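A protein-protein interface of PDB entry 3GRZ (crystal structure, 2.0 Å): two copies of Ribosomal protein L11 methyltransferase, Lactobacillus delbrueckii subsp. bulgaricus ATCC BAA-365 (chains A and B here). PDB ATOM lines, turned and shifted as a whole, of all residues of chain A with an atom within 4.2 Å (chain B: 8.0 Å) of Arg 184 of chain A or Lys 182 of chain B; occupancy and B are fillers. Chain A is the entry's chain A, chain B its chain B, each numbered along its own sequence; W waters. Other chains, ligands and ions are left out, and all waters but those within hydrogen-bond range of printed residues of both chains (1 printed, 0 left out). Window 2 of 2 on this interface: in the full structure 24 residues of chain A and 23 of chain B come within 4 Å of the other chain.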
ATOM      1  N   TYR A 162      21.468  14.719  10.361  1.00  0.00           N
ATOM      2  CA  TYR A 162      20.064  15.118  10.341  1.00  0.00           C
ATOM      3  C   TYR A 162      19.089  13.957  10.586  1.00  0.00           C
ATOM      4  O   TYR A 162      18.021  14.157  11.167  1.00  0.00           O
ATOM      5  CB  TYR A 162      19.732  15.912   9.056  1.00  0.00           C
ATOM      6  CG  TYR A 162      19.487  15.060   7.825  1.00  0.00           C
ATOM      7  CD1 TYR A 162      18.200  14.899   7.305  1.00  0.00           C
ATOM      8  CD2 TYR A 162      20.541  14.415   7.181  1.00  0.00           C
ATOM      9  CE1 TYR A 162      17.981  14.126   6.170  1.00  0.00           C
ATOM     10  CE2 TYR A 162      20.331  13.638   6.064  1.00  0.00           C
ATOM     11  CZ  TYR A 162      19.053  13.490   5.565  1.00  0.00           C
ATOM     12  OH  TYR A 162      18.856  12.709   4.451  1.00  0.00           O
ATOM     13  N   LYS A 182      17.778  25.773  15.830  1.00  0.00           N
ATOM     14  CA  LYS A 182      18.259  24.631  15.067  1.00  0.00           C
ATOM     15  C   LYS A 182      18.985  25.137  13.832  1.00  0.00           C
ATOM     16  O   LYS A 182      18.457  25.949  13.069  1.00  0.00           O
ATOM     17  CB  LYS A 182      17.098  23.726  14.666  1.00  0.00           C
ATOM     18  CG  LYS A 182      17.513  22.515  13.829  1.00  0.00           C
ATOM     19  CD  LYS A 182      16.372  21.525  13.694  1.00  0.00           C
ATOM     20  CE  LYS A 182      15.496  21.804  12.480  1.00  0.00           C
ATOM     21  NZ  LYS A 182      14.440  20.755  12.341  1.00  0.00           N
ATOM     22  N   MET A 183      20.208  24.660  13.643  1.00  0.00           N
ATOM     23  CA  MET A 183      21.033  25.045  12.523  1.00  0.00           C
ATOM     24  C   MET A 183      21.320  23.811  11.685  1.00  0.00           C
ATOM     25  O   MET A 183      21.652  22.762  12.225  1.00  0.00           O
ATOM     26  CB  MET A 183      22.362  25.619  13.021  1.00  0.00           C
ATOM     27  CG  MET A 183      22.304  26.994  13.695  1.00  0.00           C
ATOM     28  SD  MET A 183      23.876  27.345  14.543  1.00  0.00           S
ATOM     29  CE  MET A 183      23.608  26.399  16.043  1.00  0.00           C
ATOM     30  N   ARG A 184      21.204  23.928  10.368  1.00  0.00           N
ATOM     31  CA  ARG A 184      21.568  22.812   9.490  1.00  0.00           C
ATOM     32  C   ARG A 184      22.494  23.255   8.374  1.00  0.00           C
ATOM     33  O   ARG A 184      22.164  24.175   7.615  1.00  0.00           O
ATOM     34  CB  ARG A 184      20.332  22.107   8.913  1.00  0.00           C
ATOM     35  CG  ARG A 184      20.709  21.046   7.878  1.00  0.00           C
ATOM     36  CD  ARG A 184      19.618  20.050   7.610  1.00  0.00           C
ATOM     37  NE  ARG A 184      20.044  19.121   6.563  1.00  0.00           N
ATOM     38  CZ  ARG A 184      19.265  18.189   6.023  1.00  0.00           C
ATOM     39  NH1 ARG A 184      19.735  17.402   5.060  1.00  0.00           N
ATOM     40  NH2 ARG A 184      18.015  18.051   6.445  1.00  0.00           N
ATOM     41  N   ALA A 185      23.655  22.607   8.281  1.00  0.00           N
ATOM     42  CA  ALA A 185      24.576  22.828   7.156  1.00  0.00           C
ATOM     43  C   ALA A 185      24.954  21.490   6.534  1.00  0.00           C
ATOM     44  O   ALA A 185      25.573  20.648   7.190  1.00  0.00           O
ATOM     45  CB  ALA A 185      25.820  23.575   7.611  1.00  0.00           C
ATOM     46  N   GLY A 186      24.579  21.300   5.271  1.00  0.00           N
ATOM     47  CA  GLY A 186      24.618  19.975   4.653  1.00  0.00           C
ATOM     48  C   GLY A 186      23.766  19.007   5.448  1.00  0.00           C
ATOM     49  O   GLY A 186      22.586  19.263   5.686  1.00  0.00           O
ATOM     50  N   TRP A 188      24.611  18.098   8.600  1.00  0.00           N
ATOM     51  CA  TRP A 188      24.942  18.292  10.011  1.00  0.00           C
ATOM     52  C   TRP A 188      23.976  19.240  10.703  1.00  0.00           C
ATOM     53  O   TRP A 188      23.524  20.218  10.102  1.00  0.00           O
ATOM     54  CB  TRP A 188      26.369  18.828  10.146  1.00  0.00           C
ATOM     55  CG  TRP A 188      27.395  17.889   9.612  1.00  0.00           C
ATOM     56  CD1 TRP A 188      28.146  18.046   8.480  1.00  0.00           C
ATOM     57  CD2 TRP A 188      27.779  16.625  10.181  1.00  0.00           C
ATOM     58  NE1 TRP A 188      28.975  16.957   8.308  1.00  0.00           N
ATOM     59  CE2 TRP A 188      28.775  16.074   9.340  1.00  0.00           C
ATOM     60  CE3 TRP A 188      27.377  15.908  11.324  1.00  0.00           C
ATOM     61  CZ2 TRP A 188      29.391  14.841   9.611  1.00  0.00           C
ATOM     62  CZ3 TRP A 188      27.985  14.678  11.593  1.00  0.00           C
ATOM     63  CH2 TRP A 188      28.990  14.163  10.741  1.00  0.00           C
ATOM     64  N   ILE A 189      23.696  18.956  11.976  1.00  0.00           N
ATOM     65  CA  ILE A 189      22.737  19.705  12.778  1.00  0.00           C
ATOM     66  C   ILE A 189      23.474  20.270  13.991  1.00  0.00           C
ATOM     67  O   ILE A 189      24.225  19.544  14.665  1.00  0.00           O
ATOM     68  CB  ILE A 189      21.537  18.805  13.260  1.00  0.00           C
ATOM     69  CG1 ILE A 189      20.793  18.145  12.095  1.00  0.00           C
ATOM     70  CG2 ILE A 189      20.532  19.572  14.142  1.00  0.00           C
ATOM     71  CD1 ILE A 189      19.979  19.056  11.203  1.00  0.00           C
ATOM     72  N   LEU B  49      18.625  35.957  13.358  1.00  0.00           N
ATOM     73  CA  LEU B  49      18.985  34.978  12.315  1.00  0.00           C
ATOM     74  C   LEU B  49      19.787  35.650  11.214  1.00  0.00           C
ATOM     75  O   LEU B  49      20.861  35.163  10.819  1.00  0.00           O
ATOM     76  CB  LEU B  49      17.743  34.256  11.755  1.00  0.00           C
ATOM     77  CG  LEU B  49      16.920  33.450  12.782  1.00  0.00           C
ATOM     78  CD1 LEU B  49      15.803  32.652  12.128  1.00  0.00           C
ATOM     79  CD2 LEU B  49      17.816  32.549  13.635  1.00  0.00           C
ATOM     80  N   ARG B  56      28.685  35.309  10.044  1.00  0.00           N
ATOM     81  CA  ARG B  56      29.299  34.183   9.367  1.00  0.00           C
ATOM     82  C   ARG B  56      29.952  34.625   8.065  1.00  0.00           C
ATOM     83  O   ARG B  56      31.087  34.234   7.776  1.00  0.00           O
ATOM     84  CB  ARG B  56      28.255  33.090   9.129  1.00  0.00           C
ATOM     85  CG  ARG B  56      28.710  31.904   8.300  1.00  0.00           C
ATOM     86  CD  ARG B  56      27.523  30.987   8.023  1.00  0.00           C
ATOM     87  NE  ARG B  56      27.836  29.925   7.080  1.00  0.00           N
ATOM     88  CZ  ARG B  56      27.789  30.053   5.756  1.00  0.00           C
ATOM     89  NH1 ARG B  56      28.101  29.029   4.973  1.00  0.00           N
ATOM     90  NH2 ARG B  56      27.449  31.206   5.212  1.00  0.00           N
ATOM     91  N   LEU B 165       8.775  27.807   3.602  1.00  0.00           N
ATOM     92  CA  LEU B 165      10.100  27.320   3.186  1.00  0.00           C
ATOM     93  C   LEU B 165      10.178  26.465   1.889  1.00  0.00           C
ATOM     94  O   LEU B 165      11.043  26.734   1.055  1.00  0.00           O
ATOM     95  CB  LEU B 165      10.862  26.683   4.373  1.00  0.00           C
ATOM     96  CG  LEU B 165      12.307  26.202   4.173  1.00  0.00           C
ATOM     97  CD1 LEU B 165      13.254  27.316   3.679  1.00  0.00           C
ATOM     98  CD2 LEU B 165      12.822  25.559   5.449  1.00  0.00           C
ATOM     99  N   GLU B 169      12.596  27.357  -1.094  1.00  0.00           N
ATOM    100  CA  GLU B 169      13.573  26.356  -1.540  1.00  0.00           C
ATOM    101  C   GLU B 169      13.464  26.018  -3.029  1.00  0.00           C
ATOM    102  O   GLU B 169      14.473  25.879  -3.707  1.00  0.00           O
ATOM    103  CB  GLU B 169      13.456  25.079  -0.707  1.00  0.00           C
ATOM    104  CG  GLU B 169      14.035  25.199   0.698  1.00  0.00           C
ATOM    105  CD  GLU B 169      13.943  23.913   1.514  1.00  0.00           C
ATOM    106  OE1 GLU B 169      13.027  23.097   1.274  1.00  0.00           O
ATOM    107  OE2 GLU B 169      14.785  23.730   2.416  1.00  0.00           O
ATOM    108  N   ILE B 179      21.460  26.439  -0.588  1.00  0.00           N
ATOM    109  CA  ILE B 179      21.398  26.843   0.812  1.00  0.00           C
ATOM    110  C   ILE B 179      22.591  26.218   1.529  1.00  0.00           C
ATOM    111  O   ILE B 179      22.699  24.993   1.632  1.00  0.00           O
ATOM    112  CB  ILE B 179      20.066  26.394   1.473  1.00  0.00           C
ATOM    113  CG1 ILE B 179      18.871  27.037   0.761  1.00  0.00           C
ATOM    114  CG2 ILE B 179      20.061  26.709   2.972  1.00  0.00           C
ATOM    115  CD1 ILE B 179      17.498  26.488   1.204  1.00  0.00           C
ATOM    116  N   ASP B 180      23.492  27.074   1.995  1.00  0.00           N
ATOM    117  CA  ASP B 180      24.673  26.663   2.718  1.00  0.00           C
ATOM    118  C   ASP B 180      24.373  26.460   4.202  1.00  0.00           C
ATOM    119  O   ASP B 180      25.051  25.685   4.884  1.00  0.00           O
ATOM    120  CB  ASP B 180      25.766  27.722   2.565  1.00  0.00           C
ATOM    121  CG  ASP B 180      26.093  28.026   1.118  1.00  0.00           C
ATOM    122  OD1 ASP B 180      25.983  27.129   0.255  1.00  0.00           O
ATOM    123  OD2 ASP B 180      26.482  29.172   0.843  1.00  0.00           O
ATOM    124  N   LEU B 181      23.375  27.188   4.699  1.00  0.00           N
ATOM    125  CA  LEU B 181      23.011  27.163   6.116  1.00  0.00           C
ATOM    126  C   LEU B 181      21.550  27.536   6.290  1.00  0.00           C
ATOM    127  O   LEU B 181      21.081  28.536   5.757  1.00  0.00           O
ATOM    128  CB  LEU B 181      23.907  28.094   6.937  1.00  0.00           C
ATOM    129  CG  LEU B 181      23.549  28.311   8.418  1.00  0.00           C
ATOM    130  CD1 LEU B 181      23.825  27.071   9.303  1.00  0.00           C
ATOM    131  CD2 LEU B 181      24.282  29.511   8.960  1.00  0.00           C
ATOM    132  N   LYS B 182      20.836  26.688   7.014  1.00  0.00           N
ATOM    133  CA  LYS B 182      19.445  26.896   7.353  1.00  0.00           C
ATOM    134  C   LYS B 182      19.360  27.049   8.871  1.00  0.00           C
ATOM    135  O   LYS B 182      19.904  26.240   9.624  1.00  0.00           O
ATOM    136  CB  LYS B 182      18.613  25.709   6.873  1.00  0.00           C
ATOM    137  CG  LYS B 182      17.136  25.788   7.239  1.00  0.00           C
ATOM    138  CD  LYS B 182      16.352  24.625   6.633  1.00  0.00           C
ATOM    139  CE  LYS B 182      16.459  23.356   7.481  1.00  0.00           C
ATOM    140  NZ  LYS B 182      15.856  22.168   6.801  1.00  0.00           N
ATOM    141  N   MET B 183      18.706  28.108   9.324  1.00  0.00           N
ATOM    142  CA  MET B 183      18.545  28.328  10.760  1.00  0.00           C
ATOM    143  C   MET B 183      17.060  28.428  11.062  1.00  0.00           C
ATOM    144  O   MET B 183      16.319  29.013  10.292  1.00  0.00           O
ATOM    145  CB  MET B 183      19.250  29.617  11.192  1.00  0.00           C
ATOM    146  CG  MET B 183      20.769  29.578  11.188  1.00  0.00           C
ATOM    147  SD  MET B 183      21.474  31.232  11.508  1.00  0.00           S
ATOM    148  CE  MET B 183      21.224  32.018   9.939  1.00  0.00           C
ATOM    149  N   ARG B 184      16.619  27.830  12.161  1.00  0.00           N
ATOM    150  CA  ARG B 184      15.237  27.927  12.550  1.00  0.00           C
ATOM    151  C   ARG B 184      15.119  28.242  14.028  1.00  0.00           C
ATOM    152  O   ARG B 184      15.597  27.471  14.865  1.00  0.00           O
ATOM    153  CB  ARG B 184      14.466  26.645  12.212  1.00  0.00           C
ATOM    154  CG  ARG B 184      13.053  26.695  12.791  1.00  0.00           C
ATOM    155  CD  ARG B 184      12.100  25.730  12.179  1.00  0.00           C
ATOM    156  NE  ARG B 184      10.808  25.827  12.851  1.00  0.00           N
ATOM    157  CZ  ARG B 184       9.780  25.026  12.612  1.00  0.00           C
ATOM    158  NH1 ARG B 184       8.648  25.187  13.284  1.00  0.00           N
ATOM    159  NH2 ARG B 184       9.884  24.069  11.700  1.00  0.00           N
ATOM    160  N   ALA B 185      14.485  29.375  14.333  1.00  0.00           N
ATOM    161  CA  ALA B 185      14.158  29.773  15.704  1.00  0.00           C
ATOM    162  C   ALA B 185      12.654  30.047  15.816  1.00  0.00           C
ATOM    163  O   ALA B 185      12.133  30.965  15.173  1.00  0.00           O
ATOM    164  CB  ALA B 185      14.963  31.014  16.121  1.00  0.00           C
ATOM    165  N   TRP B 188      10.348  30.789  12.679  1.00  0.00           N
ATOM    166  CA  TRP B 188      11.098  31.605  11.715  1.00  0.00           C
ATOM    167  C   TRP B 188      12.337  30.922  11.180  1.00  0.00           C
ATOM    168  O   TRP B 188      13.043  30.251  11.916  1.00  0.00           O
ATOM    169  CB  TRP B 188      11.499  32.949  12.339  1.00  0.00           C
ATOM    170  CG  TRP B 188      10.324  33.734  12.760  1.00  0.00           C
ATOM    171  CD1 TRP B 188       9.919  33.985  14.045  1.00  0.00           C
ATOM    172  CD2 TRP B 188       9.355  34.339  11.903  1.00  0.00           C
ATOM    173  NE1 TRP B 188       8.769  34.727  14.036  1.00  0.00           N
ATOM    174  CE2 TRP B 188       8.399  34.963  12.735  1.00  0.00           C
ATOM    175  CE3 TRP B 188       9.207  34.429  10.506  1.00  0.00           C
ATOM    176  CZ2 TRP B 188       7.308  35.671  12.220  1.00  0.00           C
ATOM    177  CZ3 TRP B 188       8.120  35.135   9.995  1.00  0.00           C
ATOM    178  CH2 TRP B 188       7.186  35.743  10.852  1.00  0.00           C
ATOM    179  N   ILE B 189      12.598  31.140   9.899  1.00  0.00           N
ATOM    180  CA  ILE B 189      13.717  30.550   9.191  1.00  0.00           C
ATOM    181  C   ILE B 189      14.642  31.638   8.682  1.00  0.00           C
ATOM    182  O   ILE B 189      14.181  32.671   8.174  1.00  0.00           O
ATOM    183  CB  ILE B 189      13.218  29.712   7.963  1.00  0.00           C
ATOM    184  CG1 ILE B 189      12.133  28.703   8.369  1.00  0.00           C
ATOM    185  CG2 ILE B 189      14.368  29.036   7.234  1.00  0.00           C
ATOM    186  CD1 ILE B 189      12.626  27.465   9.034  1.00  0.00           C
ATOM    187  N   GLY B 190      15.947  31.404   8.818  1.00  0.00           N
ATOM    188  CA  GLY B 190      16.971  32.212   8.157  1.00  0.00           C
ATOM    189  C   GLY B 190      17.820  31.332   7.261  1.00  0.00           C
ATOM    190  O   GLY B 190      18.084  30.178   7.590  1.00  0.00           O
ATOM    191  N   LEU B 191      18.250  31.867   6.125  1.00  0.00           N
ATOM    192  CA  LEU B 191      19.071  31.103   5.178  1.00  0.00           C
ATOM    193  C   LEU B 191      20.322  31.839   4.741  1.00  0.00           C
ATOM    194  O   LEU B 191      20.257  33.027   4.410  1.00  0.00           O
ATOM    195  CB  LEU B 191      18.271  30.766   3.911  1.00  0.00           C
ATOM    196  CG  LEU B 191      16.906  30.092   4.027  1.00  0.00           C
ATOM    197  CD1 LEU B 191      16.237  30.104   2.647  1.00  0.00           C
ATOM    198  CD2 LEU B 191      17.049  28.665   4.551  1.00  0.00           C
ATOM    199  N   ALA B 192      21.446  31.123   4.725  1.00  0.00           N
ATOM    200  CA  ALA B 192      22.659  31.575   4.048  1.00  0.00           C
ATOM    201  C   ALA B 192      22.707  30.872   2.692  1.00  0.00           C
ATOM    202  O   ALA B 192      22.597  29.643   2.619  1.00  0.00           O
ATOM    203  CB  ALA B 192      23.899  31.259   4.867  1.00  0.00           C
ATOM    204  N   ILE B 193      22.867  31.667   1.639  1.00  0.00           N
ATOM    205  CA  ILE B 193      22.646  31.255   0.260  1.00  0.00           C
ATOM    206  C   ILE B 193      23.853  31.637  -0.608  1.00  0.00           C
ATOM    207  O   ILE B 193      24.446  32.699  -0.430  1.00  0.00           O
ATOM    208  CB  ILE B 193      21.343  31.914  -0.299  1.00  0.00           C
ATOM    209  CG1 ILE B 193      20.101  31.367   0.417  1.00  0.00           C
ATOM    210  CG2 ILE B 193      21.186  31.723  -1.818  1.00  0.00           C
ATOM    211  CD1 ILE B 193      18.926  32.353   0.427  1.00  0.00           C
HETATM  212  O   HOH W   1      23.014  23.035   3.512  1.00  0.00           O
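N of Arg 184 of chain B lies within hydrogen-bond range of O of Lys 182 of chain A (2.8 Å). N of Arg 184 of chain A lies within hydrogen-bond range of O of Lys 182 of chain B.
The guanidinium group of Arg 184 of chain A sits at hydrogen-bond distance from the backbone carbonyl oxygen of Gly 186 of chain A (2.7 Å). N of Asp 180 of chain B sits at hydrogen-bond distance from O of Ala 192 of chain B (2.8 Å). O of Leu 181 of chain B lies within hydrogen-bond range of N of Ala 192 of chain B (2.8 Å). The backbone NH (N) of Met 183 of chain B lies within hydrogen-bond range of the backbone carbonyl oxygen (O) of Gly 190 of chain B, at 2.8 Å.
Among the printed residues, pairs that only touch across the chains: Lys 182 of chain A with Met 183 of chain B (3.3 Å), Met 183 of chain A with Lys 182 of chain B (3.3 Å), Arg 184 of chain A with Leu 181 of chain B (3.4 Å), Ala 185 of chain A with Asp 180 of chain B (3.5 Å), Lys 182 of chain A with Lys 182 of chain B (3.7 Å) and Met 183 of chain A with Met 183 of chain B (3.9 Å).
Arg 184 of chain A touches two residues of chain B. Lys 182 of chain B touches just these residues of chain A: Lys 182 (3.7 Å), Met 183 (3.3 Å) and Arg 184 (2.8 Å). Of the printed residues of chain A, Arg 184 of chain B touches Lys 182. Printed residues of chain A within 4 Å of Leu 181 of chain B: Arg 184. Of the printed residues of chain A, Asp 180 of chain B touches Ala 185 (3.5 Å). Printed residues of chain B within 4 Å of Met 183 of chain A: Lys 182 (3.3 Å) and Met 183 (3.9 Å). Printed residues of chain B within 4 Å of Lys 182 of chain A: Lys 182 (3.7 Å), Met 183 (3.3 Å) and Arg 184 (2.8 Å). Tyr 162 of chain A touches none of the printed residues of chain B. The nearest residue of chain B that does not touch Arg 184 of chain A is Asp 180 of chain B (4.3 Å). The nearest printed residue of chain A that does not touch Lys 182 of chain B is Ala 185 of chain A (5.1 Å).
Printed residues of chain A that touch a printed residue of chain B: Lys 182, Met 183, Arg 184 and Ala 185. Hydrophobic or aromatic side chains of chain A that line the printed part of chain B: Met 183 and Ala 185. Of the 17 printed residues of chain B, 5 touch a printed residue of chain A. Hydrophobic or aromatic side chains of chain B that line the printed part of chain A: Leu 181 and Met 183. Among the printed residues, 8 pairs touch across the chains. Among the printed residues, no Asp or Glu carboxylate lies within 4 Å of a Lys or Arg side-chain nitrogen of the other chain.
Lys 182 of chain B touches its own counterpart, Lys 182 of chain A. Lys 182 of chain A touches Met 183 of chain B, and with the chains exchanged Met 183 of chain A touches Lys 182 of chain B. Lys 182 of chain A touches Arg 184 of chain B, and with the chains exchanged Arg 184 of chain A touches Lys 182 of chain B. Met 183 of chain B touches its own counterpart, Met 183 of chain A. Of the 8 pairs that touch across the chains among the printed residues, 6 have their exchanged pair printed and touching as well.
Water W1 lies within hydrogen-bond range of the backbone carbonyl oxygen (O) of Ile 179 of chain B and the backbone NH (N) of Gly 186 of chain A.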
